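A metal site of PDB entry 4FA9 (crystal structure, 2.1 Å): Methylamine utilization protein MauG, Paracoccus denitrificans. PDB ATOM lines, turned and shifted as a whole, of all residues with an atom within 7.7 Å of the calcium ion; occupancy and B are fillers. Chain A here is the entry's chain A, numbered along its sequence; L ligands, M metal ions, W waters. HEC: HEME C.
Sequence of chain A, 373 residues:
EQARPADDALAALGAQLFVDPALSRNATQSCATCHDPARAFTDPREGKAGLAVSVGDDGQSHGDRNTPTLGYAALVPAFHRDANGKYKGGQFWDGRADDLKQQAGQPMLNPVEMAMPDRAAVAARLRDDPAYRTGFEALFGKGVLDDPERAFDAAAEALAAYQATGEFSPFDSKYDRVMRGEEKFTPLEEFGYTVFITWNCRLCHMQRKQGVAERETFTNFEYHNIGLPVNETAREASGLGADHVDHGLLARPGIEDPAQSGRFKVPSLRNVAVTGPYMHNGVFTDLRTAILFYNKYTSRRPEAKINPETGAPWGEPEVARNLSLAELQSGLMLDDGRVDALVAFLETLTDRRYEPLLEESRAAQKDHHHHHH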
ATOM      1  N   ARG A  39       3.704 -27.111  -7.124  1.00  0.00           N
ATOM      2  CA  ARG A  39       3.167 -25.780  -7.239  1.00  0.00           C
ATOM      3  C   ARG A  39       1.665 -25.782  -7.442  1.00  0.00           C
ATOM      4  O   ARG A  39       1.162 -25.086  -8.271  1.00  0.00           O
ATOM      5  CB  ARG A  39       3.844 -24.971  -8.324  1.00  0.00           C
ATOM      6  CG  ARG A  39       4.001 -23.555  -7.908  1.00  0.00           C
ATOM      7  CD  ARG A  39       4.662 -22.643  -8.888  1.00  0.00           C
ATOM      8  NE  ARG A  39       3.613 -21.973  -9.572  1.00  0.00           N
ATOM      9  CZ  ARG A  39       3.459 -20.687  -9.741  1.00  0.00           C
ATOM     10  NH1 ARG A  39       4.320 -19.810  -9.318  1.00  0.00           N
ATOM     11  NH2 ARG A  39       2.394 -20.297 -10.384  1.00  0.00           N
ATOM     12  N   THR A  42       0.508 -26.270 -11.133  1.00  0.00           N
ATOM     13  CA  THR A  42       0.703 -25.183 -12.107  1.00  0.00           C
ATOM     14  C   THR A  42       2.194 -25.191 -12.440  1.00  0.00           C
ATOM     15  O   THR A  42       2.940 -26.000 -11.884  1.00  0.00           O
ATOM     16  CB  THR A  42       0.322 -23.743 -11.591  1.00  0.00           C
ATOM     17  OG1 THR A  42       1.190 -23.351 -10.513  1.00  0.00           O
ATOM     18  CG2 THR A  42      -1.120 -23.636 -11.142  1.00  0.00           C
ATOM     19  N   ASP A  43       2.590 -24.252 -13.316  1.00  0.00           N
ATOM     20  CA  ASP A  43       3.944 -24.243 -13.936  1.00  0.00           C
ATOM     21  C   ASP A  43       4.926 -23.273 -13.314  1.00  0.00           C
ATOM     22  O   ASP A  43       4.772 -22.004 -13.445  1.00  0.00           O
ATOM     23  CB  ASP A  43       3.861 -24.021 -15.437  1.00  0.00           C
ATOM     24  CG  ASP A  43       5.176 -24.416 -16.189  1.00  0.00           C
ATOM     25  OD1 ASP A  43       5.116 -24.443 -17.449  1.00  0.00           O
ATOM     26  OD2 ASP A  43       6.235 -24.686 -15.535  1.00  0.00           O
ATOM     27  N   LEU A  51       6.197 -16.266 -15.992  1.00  0.00           N
ATOM     28  CA  LEU A  51       5.411 -17.429 -15.609  1.00  0.00           C
ATOM     29  C   LEU A  51       3.992 -17.358 -16.242  1.00  0.00           C
ATOM     30  O   LEU A  51       3.098 -18.157 -15.902  1.00  0.00           O
ATOM     31  CB  LEU A  51       5.333 -17.513 -14.069  1.00  0.00           C
ATOM     32  CG  LEU A  51       6.281 -18.322 -13.172  1.00  0.00           C
ATOM     33  CD1 LEU A  51       7.496 -18.925 -13.852  1.00  0.00           C
ATOM     34  CD2 LEU A  51       6.757 -17.458 -11.986  1.00  0.00           C
ATOM     35  N   ALA A  52       3.810 -16.419 -17.182  1.00  0.00           N
ATOM     36  CA  ALA A  52       2.501 -16.097 -17.740  1.00  0.00           C
ATOM     37  C   ALA A  52       1.919 -17.232 -18.572  1.00  0.00           C
ATOM     38  O   ALA A  52       0.752 -17.546 -18.462  1.00  0.00           O
ATOM     39  CB  ALA A  52       2.505 -14.796 -18.540  1.00  0.00           C
ATOM     40  N   ASN A  66      -2.352 -18.912 -19.364  1.00  0.00           N
ATOM     41  CA  ASN A  66      -1.654 -19.320 -18.125  1.00  0.00           C
ATOM     42  C   ASN A  66      -2.160 -20.721 -17.776  1.00  0.00           C
ATOM     43  O   ASN A  66      -3.368 -21.023 -17.929  1.00  0.00           O
ATOM     44  CB  ASN A  66      -2.025 -18.302 -17.043  1.00  0.00           C
ATOM     45  CG  ASN A  66      -1.389 -18.583 -15.674  1.00  0.00           C
ATOM     46  OD1 ASN A  66      -2.121 -18.892 -14.707  1.00  0.00           O
ATOM     47  ND2 ASN A  66      -0.030 -18.428 -15.557  1.00  0.00           N
ATOM     48  N   THR A  67      -1.245 -21.575 -17.367  1.00  0.00           N
ATOM     49  CA  THR A  67      -1.577 -22.913 -16.971  1.00  0.00           C
ATOM     50  C   THR A  67      -2.254 -22.849 -15.614  1.00  0.00           C
ATOM     51  O   THR A  67      -1.633 -22.442 -14.637  1.00  0.00           O
ATOM     52  CB  THR A  67      -0.311 -23.730 -16.882  1.00  0.00           C
ATOM     53  OG1 THR A  67       0.287 -23.847 -18.188  1.00  0.00           O
ATOM     54  CG2 THR A  67      -0.607 -25.112 -16.307  1.00  0.00           C
ATOM     55  N   PRO A  68      -3.541 -23.247 -15.550  1.00  0.00           N
ATOM     56  CA  PRO A  68      -4.324 -23.236 -14.312  1.00  0.00           C
ATOM     57  C   PRO A  68      -4.053 -24.457 -13.384  1.00  0.00           C
ATOM     58  O   PRO A  68      -3.628 -25.559 -13.815  1.00  0.00           O
ATOM     59  CB  PRO A  68      -5.799 -23.269 -14.837  1.00  0.00           C
ATOM     60  CG  PRO A  68      -5.650 -24.141 -16.129  1.00  0.00           C
ATOM     61  CD  PRO A  68      -4.220 -23.974 -16.633  1.00  0.00           C
ATOM     62  N   THR A  69      -4.308 -24.281 -12.094  1.00  0.00           N
ATOM     63  CA  THR A  69      -4.252 -25.423 -11.194  1.00  0.00           C
ATOM     64  C   THR A  69      -5.226 -26.521 -11.636  1.00  0.00           C
ATOM     65  O   THR A  69      -6.277 -26.250 -12.241  1.00  0.00           O
ATOM     66  CB  THR A  69      -4.632 -25.029  -9.772  1.00  0.00           C
ATOM     67  OG1 THR A  69      -4.472 -26.169  -8.968  1.00  0.00           O
ATOM     68  CG2 THR A  69      -6.082 -24.557  -9.705  1.00  0.00           C
ATOM     69  N   TRP A  93      -9.954 -22.348 -19.813  1.00  0.00           N
ATOM     70  CA  TRP A  93     -10.432 -21.029 -19.442  1.00  0.00           C
ATOM     71  C   TRP A  93     -11.596 -20.651 -20.299  1.00  0.00           C
ATOM     72  O   TRP A  93     -12.402 -19.807 -19.902  1.00  0.00           O
ATOM     73  CB  TRP A  93      -9.351 -20.025 -19.672  1.00  0.00           C
ATOM     74  CG  TRP A  93      -8.268 -20.066 -18.767  1.00  0.00           C
ATOM     75  CD1 TRP A  93      -7.060 -20.629 -18.976  1.00  0.00           C
ATOM     76  CD2 TRP A  93      -8.218 -19.444 -17.500  1.00  0.00           C
ATOM     77  NE1 TRP A  93      -6.218 -20.382 -17.898  1.00  0.00           N
ATOM     78  CE2 TRP A  93      -6.920 -19.659 -16.972  1.00  0.00           C
ATOM     79  CE3 TRP A  93      -9.115 -18.658 -16.760  1.00  0.00           C
ATOM     80  CZ2 TRP A  93      -6.521 -19.137 -15.713  1.00  0.00           C
ATOM     81  CZ3 TRP A  93      -8.697 -18.162 -15.482  1.00  0.00           C
ATOM     82  CH2 TRP A  93      -7.432 -18.383 -15.003  1.00  0.00           C
ATOM     83  N   VAL A 272      -5.293 -19.913  -4.762  1.00  0.00           N
ATOM     84  CA  VAL A 272      -4.986 -18.745  -5.592  1.00  0.00           C
ATOM     85  C   VAL A 272      -3.701 -18.058  -5.116  1.00  0.00           C
ATOM     86  O   VAL A 272      -2.948 -17.475  -5.918  1.00  0.00           O
ATOM     87  CB  VAL A 272      -6.126 -17.710  -5.658  1.00  0.00           C
ATOM     88  CG1 VAL A 272      -6.322 -16.981  -4.316  1.00  0.00           C
ATOM     89  CG2 VAL A 272      -5.906 -16.733  -6.828  1.00  0.00           C
ATOM     90  N   VAL A 274      -0.980 -19.213  -4.361  1.00  0.00           N
ATOM     91  CA  VAL A 274       0.294 -19.777  -4.774  1.00  0.00           C
ATOM     92  C   VAL A 274       0.312 -20.110  -6.254  1.00  0.00           C
ATOM     93  O   VAL A 274       1.271 -20.742  -6.724  1.00  0.00           O
ATOM     94  CB  VAL A 274       0.708 -21.022  -3.915  1.00  0.00           C
ATOM     95  CG1 VAL A 274       0.568 -20.704  -2.443  1.00  0.00           C
ATOM     96  CG2 VAL A 274      -0.125 -22.261  -4.279  1.00  0.00           C
ATOM     97  N   THR A 275      -0.718 -19.730  -7.024  1.00  0.00           N
ATOM     98  CA  THR A 275      -0.729 -20.077  -8.464  1.00  0.00           C
ATOM     99  C   THR A 275      -0.652 -18.824  -9.347  1.00  0.00           C
ATOM    100  O   THR A 275      -1.231 -18.771 -10.443  1.00  0.00           O
ATOM    101  CB  THR A 275      -2.012 -20.794  -8.767  1.00  0.00           C
ATOM    102  OG1 THR A 275      -3.059 -19.921  -8.348  1.00  0.00           O
ATOM    103  CG2 THR A 275      -2.097 -22.035  -7.927  1.00  0.00           C
ATOM    104  N   GLY A 276       0.017 -17.800  -8.847  1.00  0.00           N
ATOM    105  CA  GLY A 276       0.365 -16.613  -9.676  1.00  0.00           C
ATOM    106  C   GLY A 276       1.272 -16.965 -10.855  1.00  0.00           C
ATOM    107  O   GLY A 276       1.997 -17.981 -10.826  1.00  0.00           O
ATOM    108  N   PRO A 277       1.261 -16.150 -11.904  1.00  0.00           N
ATOM    109  CA  PRO A 277       0.499 -14.954 -12.104  1.00  0.00           C
ATOM    110  C   PRO A 277      -0.980 -15.304 -12.403  1.00  0.00           C
ATOM    111  O   PRO A 277      -1.360 -16.468 -12.425  1.00  0.00           O
ATOM    112  CB  PRO A 277       1.217 -14.291 -13.289  1.00  0.00           C
ATOM    113  CG  PRO A 277       1.956 -15.377 -13.981  1.00  0.00           C
ATOM    114  CD  PRO A 277       1.923 -16.589 -13.167  1.00  0.00           C
ATOM    115  N   TYR A 278      -1.786 -14.281 -12.587  1.00  0.00           N
ATOM    116  CA  TYR A 278      -3.226 -14.391 -12.419  1.00  0.00           C
ATOM    117  C   TYR A 278      -3.881 -14.045 -13.723  1.00  0.00           C
ATOM    118  O   TYR A 278      -3.242 -13.418 -14.563  1.00  0.00           O
ATOM    119  CB  TYR A 278      -3.639 -13.464 -11.264  1.00  0.00           C
ATOM    120  CG  TYR A 278      -3.043 -13.955  -9.973  1.00  0.00           C
ATOM    121  CD1 TYR A 278      -1.920 -13.348  -9.420  1.00  0.00           C
ATOM    122  CD2 TYR A 278      -3.507 -15.114  -9.372  1.00  0.00           C
ATOM    123  CE1 TYR A 278      -1.330 -13.889  -8.277  1.00  0.00           C
ATOM    124  CE2 TYR A 278      -2.961 -15.612  -8.229  1.00  0.00           C
ATOM    125  CZ  TYR A 278      -1.862 -15.009  -7.698  1.00  0.00           C
ATOM    126  OH  TYR A 278      -1.287 -15.560  -6.565  1.00  0.00           O
ATOM    127  N   MET A 279      -5.163 -14.408 -13.826  1.00  0.00           N
ATOM    128  CA  MET A 279      -6.040 -14.280 -15.007  1.00  0.00           C
ATOM    129  C   MET A 279      -5.609 -15.228 -16.083  1.00  0.00           C
ATOM    130  O   MET A 279      -4.505 -15.888 -16.015  1.00  0.00           O
ATOM    131  CB  MET A 279      -6.155 -12.837 -15.521  1.00  0.00           C
ATOM    132  CG  MET A 279      -6.537 -11.845 -14.397  1.00  0.00           C
ATOM    133  SD  MET A 279      -8.027 -12.282 -13.464  1.00  0.00           S
ATOM    134  CE  MET A 279      -7.935 -10.943 -12.246  1.00  0.00           C
ATOM    135  N   HIS A 280      -6.460 -15.289 -17.089  1.00  0.00           N
ATOM    136  CA  HIS A 280      -6.364 -16.293 -18.122  1.00  0.00           C
ATOM    137  C   HIS A 280      -5.024 -16.153 -18.878  1.00  0.00           C
ATOM    138  O   HIS A 280      -4.596 -17.087 -19.548  1.00  0.00           O
ATOM    139  CB  HIS A 280      -7.602 -16.214 -19.060  1.00  0.00           C
ATOM    140  CG  HIS A 280      -7.620 -14.962 -19.901  1.00  0.00           C
ATOM    141  ND1 HIS A 280      -8.441 -13.889 -19.635  1.00  0.00           N
ATOM    142  CD2 HIS A 280      -6.867 -14.600 -20.976  1.00  0.00           C
ATOM    143  CE1 HIS A 280      -8.206 -12.921 -20.505  1.00  0.00           C
ATOM    144  NE2 HIS A 280      -7.257 -13.331 -21.335  1.00  0.00           N
ATOM    145  N   ASN A 281      -4.359 -15.024 -18.772  1.00  0.00           N
ATOM    146  CA  ASN A 281      -3.176 -14.768 -19.598  1.00  0.00           C
ATOM    147  C   ASN A 281      -1.999 -14.411 -18.702  1.00  0.00           C
ATOM    148  O   ASN A 281      -0.975 -13.949 -19.185  1.00  0.00           O
ATOM    149  CB  ASN A 281      -3.435 -13.652 -20.621  1.00  0.00           C
ATOM    150  CG  ASN A 281      -3.833 -12.321 -19.927  1.00  0.00           C
ATOM    151  OD1 ASN A 281      -3.755 -12.226 -18.702  1.00  0.00           O
ATOM    152  ND2 ASN A 281      -4.266 -11.340 -20.694  1.00  0.00           N
ATOM    153  N   GLY A 282      -2.187 -14.624 -17.405  1.00  0.00           N
ATOM    154  CA  GLY A 282      -1.133 -14.445 -16.434  1.00  0.00           C
ATOM    155  C   GLY A 282      -0.676 -13.006 -16.329  1.00  0.00           C
ATOM    156  O   GLY A 282       0.449 -12.760 -15.910  1.00  0.00           O
ATOM    157  N   PHE A 284      -1.118 -10.400 -14.437  1.00  0.00           N
ATOM    158  CA  PHE A 284      -0.751  -9.846 -13.120  1.00  0.00           C
ATOM    159  C   PHE A 284       0.034 -10.879 -12.331  1.00  0.00           C
ATOM    160  O   PHE A 284      -0.479 -11.975 -12.055  1.00  0.00           O
ATOM    161  CB  PHE A 284      -2.010  -9.492 -12.306  1.00  0.00           C
ATOM    162  CG  PHE A 284      -2.965  -8.632 -13.036  1.00  0.00           C
ATOM    163  CD1 PHE A 284      -2.503  -7.521 -13.772  1.00  0.00           C
ATOM    164  CD2 PHE A 284      -4.328  -8.896 -12.993  1.00  0.00           C
ATOM    165  CE1 PHE A 284      -3.368  -6.723 -14.470  1.00  0.00           C
ATOM    166  CE2 PHE A 284      -5.195  -8.089 -13.677  1.00  0.00           C
ATOM    167  CZ  PHE A 284      -4.696  -6.973 -14.431  1.00  0.00           C
HETATM  168 FE   HEC L   1     -12.743 -12.442  -9.803  1.00  0.00          FE
HETATM  169  CHA HEC L   1     -10.327 -13.975 -11.702  1.00  0.00           C
HETATM  170  CHB HEC L   1     -10.709 -12.342  -7.168  1.00  0.00           C
HETATM  171  CHC HEC L   1     -14.915 -10.202  -8.291  1.00  0.00           C
HETATM  172  CHD HEC L   1     -15.116 -13.242 -12.061  1.00  0.00           C
HETATM  173  NA  HEC L   1     -10.800 -13.052  -9.472  1.00  0.00           N
HETATM  174  C1A HEC L   1      -9.999 -13.673 -10.319  1.00  0.00           C
HETATM  175  C2A HEC L   1      -8.637 -13.861  -9.813  1.00  0.00           C
HETATM  176  C3A HEC L   1      -8.692 -13.385  -8.507  1.00  0.00           C
HETATM  177  C4A HEC L   1     -10.096 -12.898  -8.382  1.00  0.00           C
HETATM  178  CMA HEC L   1      -7.615 -13.396  -7.478  1.00  0.00           C
HETATM  179  CAA HEC L   1      -7.568 -14.536 -10.613  1.00  0.00           C
HETATM  180  CBA HEC L   1      -7.607 -15.983 -10.090  1.00  0.00           C
HETATM  181  CGA HEC L   1      -6.704 -16.835 -10.980  1.00  0.00           C
HETATM  182  O1A HEC L   1      -6.085 -16.250 -11.914  1.00  0.00           O
HETATM  183  O2A HEC L   1      -6.588 -18.081 -10.752  1.00  0.00           O
HETATM  184  NB  HEC L   1     -12.819 -11.430  -8.037  1.00  0.00           N
HETATM  185  C1B HEC L   1     -11.908 -11.521  -7.070  1.00  0.00           C
HETATM  186  C2B HEC L   1     -12.189 -10.697  -5.905  1.00  0.00           C
HETATM  187  C3B HEC L   1     -13.402 -10.078  -6.226  1.00  0.00           C
HETATM  188  C4B HEC L   1     -13.730 -10.601  -7.549  1.00  0.00           C
HETATM  189  CMB HEC L   1     -11.296 -10.692  -4.677  1.00  0.00           C
HETATM  190  CAB HEC L   1     -14.276  -9.100  -5.468  1.00  0.00           C
HETATM  191  CBB HEC L   1     -13.370  -7.925  -5.377  1.00  0.00           C
HETATM  192  NC  HEC L   1     -14.707 -11.835 -10.120  1.00  0.00           N
HETATM  193  C1C HEC L   1     -15.428 -10.922  -9.445  1.00  0.00           C
HETATM  194  C2C HEC L   1     -16.760 -10.664 -10.026  1.00  0.00           C
HETATM  195  C3C HEC L   1     -16.832 -11.538 -11.106  1.00  0.00           C
HETATM  196  C4C HEC L   1     -15.517 -12.205 -11.121  1.00  0.00           C
HETATM  197  CMC HEC L   1     -17.758  -9.638  -9.527  1.00  0.00           C
HETATM  198  CAC HEC L   1     -17.987 -11.769 -12.081  1.00  0.00           C
HETATM  199  CBC HEC L   1     -18.453 -10.480 -12.678  1.00  0.00           C
HETATM  200  ND  HEC L   1     -12.689 -13.433 -11.558  1.00  0.00           N
HETATM  201  C1D HEC L   1     -13.744 -13.588 -12.428  1.00  0.00           C
HETATM  202  C2D HEC L   1     -13.384 -14.173 -13.729  1.00  0.00           C
HETATM  203  C3D HEC L   1     -12.014 -14.377 -13.593  1.00  0.00           C
HETATM  204  C4D HEC L   1     -11.676 -13.900 -12.238  1.00  0.00           C
HETATM  205  CMD HEC L   1     -14.266 -14.467 -14.887  1.00  0.00           C
HETATM  206  CAD HEC L   1     -11.019 -14.860 -14.584  1.00  0.00           C
HETATM  207  CBD HEC L   1     -11.031 -13.634 -15.491  1.00  0.00           C
HETATM  208  CGD HEC L   1     -10.098 -13.866 -16.668  1.00  0.00           C
HETATM  209  O1D HEC L   1      -8.932 -14.262 -16.401  1.00  0.00           O
HETATM  210  O2D HEC L   1     -10.516 -13.621 -17.829  1.00  0.00           O
HETATM  211 CA    CA M   1      -2.148 -18.606 -12.436  1.00  0.00          CA
HETATM  212  O   HOH W   1       0.192 -19.346 -12.864  1.00  0.00           O
HETATM  213  O   HOH W   2      -3.749 -18.672 -10.629  1.00  0.00           O
HETATM  214  O   HOH W   3      -4.203 -17.767 -13.520  1.00  0.00           O
HETATM  215  O   HOH W   4      -2.498 -20.973 -12.395  1.00  0.00           O
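The calcium ion is bound by the backbone carbonyl oxygen of Thr 275 (2.2 Å), the backbone carbonyl oxygen of Pro 277 (2.3 Å), the side-chain amide oxygen of Asn 66 (2.3 Å), water W4 (2.4 Å), water W2 (2.4 Å), water W3 (2.5 Å) and water W1 (2.5 Å). The calcium ion has seven donor atoms within binding distance.
The backbone NH of Met 279 lies within hydrogen-bond range of an oxygen (O1A) of the ligand (2.8 Å). The backbone NH (N) of His 280 lies within hydrogen-bond range of an oxygen (O1D) of the ligand (2.8 Å). A ring nitrogen (ND1) of His 280 sits at hydrogen-bond distance from an oxygen (O2D) of the ligand.
O of Val 272 is in hydrogen-bond range of OG1 of Thr 275, at 3.4 Å. The backbone carbonyl oxygen (O) of Asn 66 is in hydrogen-bond range of the indole nitrogen (NE1) of Trp 93. The side-chain amide nitrogen of Asn 66 is in hydrogen-bond range of the backbone carbonyl oxygen of Leu 51 (3.2 Å). ND2 of Asn 66 lies close to O of Ala 52. N of Asn 66 lies within hydrogen-bond range of O of His 280 (2.9 Å).
Three residues have an atom within 4 Å of the calcium ion: Asn 66, Thr 275 and Pro 277. The nearest printed residue that does not touch the calcium ion is Gly 276 (4.1 Å).
Water W2 lies within hydrogen-bond range of the side-chain hydroxyl (OG1) of Thr 275 (2.7 Å) and an oxygen (O2A) of the ligand (2.9 Å). Water W1 lies within hydrogen-bond range of the side-chain amide nitrogen of Asn 66 (2.9 Å), the backbone carbonyl oxygen of Gly 276 (3.0 Å) and the guanidinium group of Arg 39 (3.5 Å). Water W3 lies within hydrogen-bond range of an oxygen (O1A) of the ligand and the backbone carbonyl oxygen of Met 279.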
